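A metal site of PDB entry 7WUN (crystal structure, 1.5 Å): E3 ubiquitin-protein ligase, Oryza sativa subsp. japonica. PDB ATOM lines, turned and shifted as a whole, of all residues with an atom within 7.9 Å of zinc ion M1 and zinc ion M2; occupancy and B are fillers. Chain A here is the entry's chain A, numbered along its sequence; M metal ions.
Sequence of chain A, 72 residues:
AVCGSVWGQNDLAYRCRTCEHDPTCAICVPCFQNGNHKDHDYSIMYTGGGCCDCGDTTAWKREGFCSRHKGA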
ATOM      1  N   ALA A   1      13.612  24.833  31.740  1.00  0.00           N
ATOM      2  CA  ALA A   1      13.173  23.522  31.276  1.00  0.00           C
ATOM      3  C   ALA A   1      13.218  23.417  29.751  1.00  0.00           C
ATOM      4  O   ALA A   1      13.744  22.446  29.194  1.00  0.00           O
ATOM      5  CB  ALA A   1      11.764  23.230  31.772  1.00  0.00           C
ATOM      6  N   VAL A   2      12.638  24.419  29.093  1.00  0.00           N
ATOM      7  CA  VAL A   2      12.649  24.556  27.647  1.00  0.00           C
ATOM      8  C   VAL A   2      13.318  25.882  27.315  1.00  0.00           C
ATOM      9  O   VAL A   2      12.935  26.925  27.855  1.00  0.00           O
ATOM     10  CB  VAL A   2      11.218  24.510  27.073  1.00  0.00           C
ATOM     11  CG1 VAL A   2      11.214  24.942  25.599  1.00  0.00           C
ATOM     12  CG2 VAL A   2      10.638  23.128  27.236  1.00  0.00           C
ATOM     13  N   CYS A   3      14.301  25.837  26.421  1.00  0.00           N
ATOM     14  CA  CYS A   3      15.078  27.026  26.087  1.00  0.00           C
ATOM     15  C   CYS A   3      14.173  28.169  25.645  1.00  0.00           C
ATOM     16  O   CYS A   3      13.384  28.026  24.710  1.00  0.00           O
ATOM     17  CB  CYS A   3      16.068  26.696  24.968  1.00  0.00           C
ATOM     18  SG  CYS A   3      17.122  28.092  24.492  1.00  0.00           S
ATOM     19  N   GLY A   4      14.302  29.313  26.302  1.00  0.00           N
ATOM     20  CA  GLY A   4      13.442  30.423  25.925  1.00  0.00           C
ATOM     21  C   GLY A   4      14.001  31.327  24.841  1.00  0.00           C
ATOM     22  O   GLY A   4      13.546  32.472  24.708  1.00  0.00           O
ATOM     23  N   SER A   5      14.962  30.862  24.048  1.00  0.00           N
ATOM     24  CA  SER A   5      15.652  31.777  23.154  1.00  0.00           C
ATOM     25  C   SER A   5      14.808  32.071  21.925  1.00  0.00           C
ATOM     26  O   SER A   5      14.171  31.177  21.355  1.00  0.00           O
ATOM     27  CB  SER A   5      17.019  31.236  22.751  1.00  0.00           C
ATOM     28  OG  SER A   5      17.853  32.307  22.321  1.00  0.00           O
ATOM     29  N   VAL A   6      14.793  33.327  21.545  1.00  0.00           N
ATOM     30  CA  VAL A   6      14.107  33.770  20.342  1.00  0.00           C
ATOM     31  C   VAL A   6      15.126  34.365  19.404  1.00  0.00           C
ATOM     32  O   VAL A   6      16.144  34.934  19.829  1.00  0.00           O
ATOM     33  CB  VAL A   6      12.978  34.776  20.649  1.00  0.00           C
ATOM     34  CG1 VAL A   6      12.054  34.209  21.701  1.00  0.00           C
ATOM     35  CG2 VAL A   6      13.582  36.070  21.151  1.00  0.00           C
ATOM     36  N   TRP A   7      14.881  34.216  18.114  1.00  0.00           N
ATOM     37  CA  TRP A   7      15.755  34.830  17.118  1.00  0.00           C
ATOM     38  C   TRP A   7      14.919  35.396  15.984  1.00  0.00           C
ATOM     39  O   TRP A   7      13.734  35.093  15.850  1.00  0.00           O
ATOM     40  CB  TRP A   7      16.815  33.843  16.595  1.00  0.00           C
ATOM     41  CG  TRP A   7      16.267  32.699  15.858  1.00  0.00           C
ATOM     42  CD1 TRP A   7      16.046  32.622  14.498  1.00  0.00           C
ATOM     43  CD2 TRP A   7      15.902  31.423  16.402  1.00  0.00           C
ATOM     44  NE1 TRP A   7      15.541  31.382  14.178  1.00  0.00           N
ATOM     45  CE2 TRP A   7      15.447  30.635  15.324  1.00  0.00           C
ATOM     46  CE3 TRP A   7      15.907  30.881  17.692  1.00  0.00           C
ATOM     47  CZ2 TRP A   7      14.993  29.322  15.503  1.00  0.00           C
ATOM     48  CZ3 TRP A   7      15.457  29.575  17.856  1.00  0.00           C
ATOM     49  CH2 TRP A   7      15.016  28.818  16.764  1.00  0.00           C
ATOM     50  N   ALA A  26      13.108  23.769  15.325  1.00  0.00           N
ATOM     51  CA  ALA A  26      14.447  24.335  15.244  1.00  0.00           C
ATOM     52  C   ALA A  26      14.992  24.571  16.642  1.00  0.00           C
ATOM     53  O   ALA A  26      14.228  24.787  17.587  1.00  0.00           O
ATOM     54  CB  ALA A  26      14.465  25.650  14.453  1.00  0.00           C
ATOM     55  N   ILE A  27      16.323  24.558  16.755  1.00  0.00           N
ATOM     56  CA  ILE A  27      16.987  24.943  18.004  1.00  0.00           C
ATOM     57  C   ILE A  27      18.025  26.020  17.738  1.00  0.00           C
ATOM     58  O   ILE A  27      18.578  26.140  16.635  1.00  0.00           O
ATOM     59  CB  ILE A  27      17.620  23.742  18.740  1.00  0.00           C
ATOM     60  CG1 ILE A  27      18.755  23.097  17.939  1.00  0.00           C
ATOM     61  CG2 ILE A  27      16.554  22.709  19.115  1.00  0.00           C
ATOM     62  CD1 ILE A  27      19.450  21.996  18.739  1.00  0.00           C
ATOM     63  N   CYS A  28      18.264  26.841  18.756  1.00  0.00           N
ATOM     64  CA  CYS A  28      19.220  27.921  18.620  1.00  0.00           C
ATOM     65  C   CYS A  28      20.636  27.385  18.485  1.00  0.00           C
ATOM     66  O   CYS A  28      20.941  26.231  18.808  1.00  0.00           O
ATOM     67  CB  CYS A  28      19.103  28.868  19.831  1.00  0.00           C
ATOM     68  SG  CYS A  28      19.696  28.219  21.432  1.00  0.00           S
ATOM     69  N   VAL A  29      21.533  28.247  17.988  1.00  0.00           N
ATOM     70  CA  VAL A  29      22.909  27.816  17.760  1.00  0.00           C
ATOM     71  C   VAL A  29      23.566  27.311  19.049  1.00  0.00           C
ATOM     72  O   VAL A  29      24.165  26.227  19.031  1.00  0.00           O
ATOM     73  CB  VAL A  29      23.719  28.943  17.093  1.00  0.00           C
ATOM     74  CG1 VAL A  29      25.205  28.645  17.157  1.00  0.00           C
ATOM     75  CG2 VAL A  29      23.250  29.134  15.663  1.00  0.00           C
ATOM     76  N   PRO A  30      23.481  28.004  20.188  1.00  0.00           N
ATOM     77  CA  PRO A  30      24.112  27.446  21.395  1.00  0.00           C
ATOM     78  C   PRO A  30      23.543  26.108  21.841  1.00  0.00           C
ATOM     79  O   PRO A  30      24.299  25.252  22.308  1.00  0.00           O
ATOM     80  CB  PRO A  30      23.918  28.538  22.447  1.00  0.00           C
ATOM     81  CG  PRO A  30      23.557  29.758  21.721  1.00  0.00           C
ATOM     82  CD  PRO A  30      23.024  29.393  20.375  1.00  0.00           C
ATOM     83  N   CYS A  31      22.224  25.907  21.710  1.00  0.00           N
ATOM     84  CA  CYS A  31      21.675  24.591  22.066  1.00  0.00           C
ATOM     85  C   CYS A  31      22.189  23.507  21.135  1.00  0.00           C
ATOM     86  O   CYS A  31      22.441  22.382  21.571  1.00  0.00           O
ATOM     87  CB  CYS A  31      20.149  24.639  22.050  1.00  0.00           C
ATOM     88  SG  CYS A  31      19.513  25.430  23.514  1.00  0.00           S
ATOM     89  N   PHE A  32      22.358  23.821  19.852  1.00  0.00           N
ATOM     90  CA  PHE A  32      22.940  22.823  18.960  1.00  0.00           C
ATOM     91  C   PHE A  32      24.367  22.493  19.380  1.00  0.00           C
ATOM     92  O   PHE A  32      24.750  21.320  19.476  1.00  0.00           O
ATOM     93  CB  PHE A  32      22.931  23.321  17.518  1.00  0.00           C
ATOM     94  CG  PHE A  32      23.467  22.304  16.555  1.00  0.00           C
ATOM     95  CD1 PHE A  32      22.663  21.267  16.094  1.00  0.00           C
ATOM     96  CD2 PHE A  32      24.801  22.329  16.202  1.00  0.00           C
ATOM     97  CE1 PHE A  32      23.167  20.298  15.226  1.00  0.00           C
ATOM     98  CE2 PHE A  32      25.313  21.348  15.330  1.00  0.00           C
ATOM     99  CZ  PHE A  32      24.506  20.347  14.860  1.00  0.00           C
ATOM    100  N   ASN A  34      25.833  22.719  22.218  1.00  0.00           N
ATOM    101  CA  ASN A  34      25.939  22.009  23.475  1.00  0.00           C
ATOM    102  C   ASN A  34      25.168  20.692  23.495  1.00  0.00           C
ATOM    103  O   ASN A  34      24.960  20.110  24.568  1.00  0.00           O
ATOM    104  CB  ASN A  34      25.484  22.912  24.616  1.00  0.00           C
ATOM    105  CG  ASN A  34      26.493  23.992  24.915  1.00  0.00           C
ATOM    106  OD1 ASN A  34      27.694  23.789  24.739  1.00  0.00           O
ATOM    107  ND2 ASN A  34      26.022  25.140  25.352  1.00  0.00           N
ATOM    108  N   GLY A  35      24.751  20.183  22.329  1.00  0.00           N
ATOM    109  CA  GLY A  35      24.116  18.891  22.217  1.00  0.00           C
ATOM    110  C   GLY A  35      24.911  17.956  21.319  1.00  0.00           C
ATOM    111  O   GLY A  35      26.001  18.285  20.841  1.00  0.00           O
ATOM    112  N   CYS A  51      11.534  30.412  17.862  1.00  0.00           N
ATOM    113  CA  CYS A  51      11.728  30.172  19.287  1.00  0.00           C
ATOM    114  C   CYS A  51      12.334  28.784  19.452  1.00  0.00           C
ATOM    115  O   CYS A  51      11.904  27.837  18.787  1.00  0.00           O
ATOM    116  CB  CYS A  51      10.431  30.219  20.067  1.00  0.00           C
ATOM    117  SG  CYS A  51       9.582  31.779  20.073  1.00  0.00           S
ATOM    118  N   CYS A  52      13.304  28.662  20.358  1.00  0.00           N
ATOM    119  CA  CYS A  52      14.041  27.407  20.458  1.00  0.00           C
ATOM    120  C   CYS A  52      13.164  26.282  21.002  1.00  0.00           C
ATOM    121  O   CYS A  52      12.389  26.480  21.954  1.00  0.00           O
ATOM    122  CB  CYS A  52      15.265  27.601  21.331  1.00  0.00           C
ATOM    123  SG  CYS A  52      16.335  26.177  21.385  1.00  0.00           S
ATOM    124  N   ASP A  53      13.300  25.090  20.413  1.00  0.00           N
ATOM    125  CA  ASP A  53      12.545  23.927  20.856  1.00  0.00           C
ATOM    126  C   ASP A  53      13.322  23.020  21.802  1.00  0.00           C
ATOM    127  O   ASP A  53      12.797  21.981  22.220  1.00  0.00           O
ATOM    128  CB  ASP A  53      12.100  23.112  19.632  1.00  0.00           C
ATOM    129  CG  ASP A  53      11.074  23.851  18.788  1.00  0.00           C
ATOM    130  OD1 ASP A  53      10.216  24.562  19.362  1.00  0.00           O
ATOM    131  OD2 ASP A  53      11.154  23.741  17.556  1.00  0.00           O
ATOM    132  N   CYS A  54      14.548  23.402  22.172  1.00  0.00           N
ATOM    133  CA  CYS A  54      15.381  22.528  22.985  1.00  0.00           C
ATOM    134  C   CYS A  54      14.775  22.367  24.367  1.00  0.00           C
ATOM    135  O   CYS A  54      14.500  23.358  25.058  1.00  0.00           O
ATOM    136  CB  CYS A  54      16.799  23.072  23.087  1.00  0.00           C
ATOM    137  SG  CYS A  54      17.896  22.040  24.019  1.00  0.00           S
ATOM    138  N   GLY A  55      14.583  21.114  24.776  1.00  0.00           N
ATOM    139  CA  GLY A  55      13.954  20.767  26.036  1.00  0.00           C
ATOM    140  C   GLY A  55      12.483  20.404  25.935  1.00  0.00           C
ATOM    141  O   GLY A  55      11.932  19.866  26.899  1.00  0.00           O
ATOM    142  N   GLY A  64      18.269  14.688  21.561  1.00  0.00           N
ATOM    143  CA  GLY A  64      18.740  15.901  20.938  1.00  0.00           C
ATOM    144  C   GLY A  64      18.733  17.144  21.811  1.00  0.00           C
ATOM    145  O   GLY A  64      19.073  18.219  21.304  1.00  0.00           O
ATOM    146  N   PHE A  65      18.374  17.030  23.088  1.00  0.00           N
ATOM    147  CA  PHE A  65      18.455  18.159  24.011  1.00  0.00           C
ATOM    148  C   PHE A  65      19.907  18.472  24.323  1.00  0.00           C
ATOM    149  O   PHE A  65      20.745  17.574  24.470  1.00  0.00           O
ATOM    150  CB  PHE A  65      17.739  17.843  25.325  1.00  0.00           C
ATOM    151  CG  PHE A  65      16.250  17.658  25.202  1.00  0.00           C
ATOM    152  CD1 PHE A  65      15.566  17.967  24.039  1.00  0.00           C
ATOM    153  CD2 PHE A  65      15.521  17.208  26.295  1.00  0.00           C
ATOM    154  CE1 PHE A  65      14.192  17.803  23.956  1.00  0.00           C
ATOM    155  CE2 PHE A  65      14.140  17.041  26.236  1.00  0.00           C
ATOM    156  CZ  PHE A  65      13.474  17.339  25.060  1.00  0.00           C
ATOM    157  N   CYS A  66      20.213  19.761  24.449  1.00  0.00           N
ATOM    158  CA  CYS A  66      21.554  20.115  24.875  1.00  0.00           C
ATOM    159  C   CYS A  66      21.720  19.805  26.356  1.00  0.00           C
ATOM    160  O   CYS A  66      20.777  19.419  27.055  1.00  0.00           O
ATOM    161  CB  CYS A  66      21.849  21.595  24.575  1.00  0.00           C
ATOM    162  SG  CYS A  66      21.241  22.771  25.806  1.00  0.00           S
ATOM    163  N   SER A  67      22.954  19.956  26.845  1.00  0.00           N
ATOM    164  CA  SER A  67      23.256  19.624  28.231  1.00  0.00           C
ATOM    165  C   SER A  67      22.524  20.509  29.232  1.00  0.00           C
ATOM    166  O   SER A  67      22.392  20.116  30.393  1.00  0.00           O
ATOM    167  CB  SER A  67      24.754  19.731  28.459  1.00  0.00           C
ATOM    168  OG  SER A  67      25.208  21.011  28.041  1.00  0.00           O
ATOM    169  N   ARG A  68      22.043  21.681  28.808  1.00  0.00           N
ATOM    170  CA  ARG A  68      21.488  22.663  29.727  1.00  0.00           C
ATOM    171  C   ARG A  68      19.967  22.649  29.782  1.00  0.00           C
ATOM    172  O   ARG A  68      19.394  23.254  30.697  1.00  0.00           O
ATOM    173  CB  ARG A  68      21.980  24.072  29.339  1.00  0.00           C
ATOM    174  CG  ARG A  68      23.475  24.219  29.485  1.00  0.00           C
ATOM    175  CD  ARG A  68      23.994  25.611  29.126  1.00  0.00           C
ATOM    176  NE  ARG A  68      23.407  26.640  29.964  1.00  0.00           N
ATOM    177  CZ  ARG A  68      22.412  27.433  29.590  1.00  0.00           C
ATOM    178  NH1 ARG A  68      21.930  27.406  28.361  1.00  0.00           N
ATOM    179  NH2 ARG A  68      21.898  28.297  30.469  1.00  0.00           N
ATOM    180  N   HIS A  69      19.315  21.982  28.857  1.00  0.00           N
ATOM    181  CA  HIS A  69      17.875  21.767  28.916  1.00  0.00           C
ATOM    182  C   HIS A  69      17.588  20.277  28.801  1.00  0.00           C
ATOM    183  O   HIS A  69      16.654  19.850  28.119  1.00  0.00           O
ATOM    184  CB  HIS A  69      17.170  22.592  27.822  1.00  0.00           C
ATOM    185  CG  HIS A  69      17.633  24.020  27.746  1.00  0.00           C
ATOM    186  ND1 HIS A  69      18.485  24.475  26.763  1.00  0.00           N
ATOM    187  CD2 HIS A  69      17.376  25.077  28.544  1.00  0.00           C
ATOM    188  CE1 HIS A  69      18.728  25.764  26.956  1.00  0.00           C
ATOM    189  NE2 HIS A  69      18.070  26.157  28.039  1.00  0.00           N
ATOM    190  N   LYS A  70      18.429  19.459  29.444  1.00  0.00           N
ATOM    191  CA  LYS A  70      18.246  18.000  29.513  1.00  0.00           C
ATOM    192  C   LYS A  70      17.631  17.614  30.845  1.00  0.00           C
ATOM    193  O   LYS A  70      16.710  18.270  31.316  1.00  0.00           O
ATOM    194  CB  LYS A  70      19.574  17.246  29.325  1.00  0.00           C
ATOM    195  CG  LYS A  70      19.788  16.714  27.906  1.00  0.00           C
ATOM    196  CD  LYS A  70      20.531  15.398  27.842  1.00  0.00           C
ATOM    197  CE  LYS A  70      19.597  14.255  27.420  1.00  0.00           C
ATOM    198  NZ  LYS A  70      20.337  12.975  27.170  1.00  0.00           N
HETATM  199 ZN    ZN M   1      18.049  27.089  22.656  1.00  0.00          ZN
HETATM  200 ZN    ZN M   2      19.226  23.620  25.044  1.00  0.00          ZN
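Of the 28 residues printed, 4 come within 4 Å of zinc ion M2.
The nearest printed residue that does not touch zinc ion M2 is Cys 3 (4.4 Å).
Zinc ion M2 is bound by ND1 of His 69 (2.1 Å).
The side-chain sulfur (SG) of Cys 54 is bound to zinc ion M2, at 2.3 Å.
Zinc ion M2 is bound by the side-chain sulfur (SG) of Cys 66, at 2.3 Å.
The side-chain sulfur (SG) of Cys 31 is bound to zinc ion M2.
N of Cys 54 lies close to SG of Cys 52 (3.4 Å).
N of Arg 68 sits close to SG of Cys 66 (3.3 Å).
SG of Cys 3 sits close to N of Ser 5 (3.5 Å).
O of Ser 5 is in hydrogen-bond range of N of Cys 52 (2.8 Å).
O of Cys 54 sits at hydrogen-bond distance from N of Cys 3 (2.8 Å).
Zinc ion M1 is bound by SG of Cys 3, at 2.3 Å.
Zinc ion M1 is bound by SG of Cys 52, 2.3 Å away.
Zinc ion M1 is bound by the side-chain sulfur (SG) of Cys 28 (2.3 Å).
SG of Cys 31 is bound to zinc ion M1 (2.4 Å).
Four residues have an atom within 4 Å of zinc ion M1: Cys 3, Cys 28, Cys 31 and Cys 52.
Along chain A the residues within 4 Å of zinc ion M1 span positions 3 to 52.
The nearest printed residue that does not touch zinc ion M1 is Cys 54 (4.2 Å).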
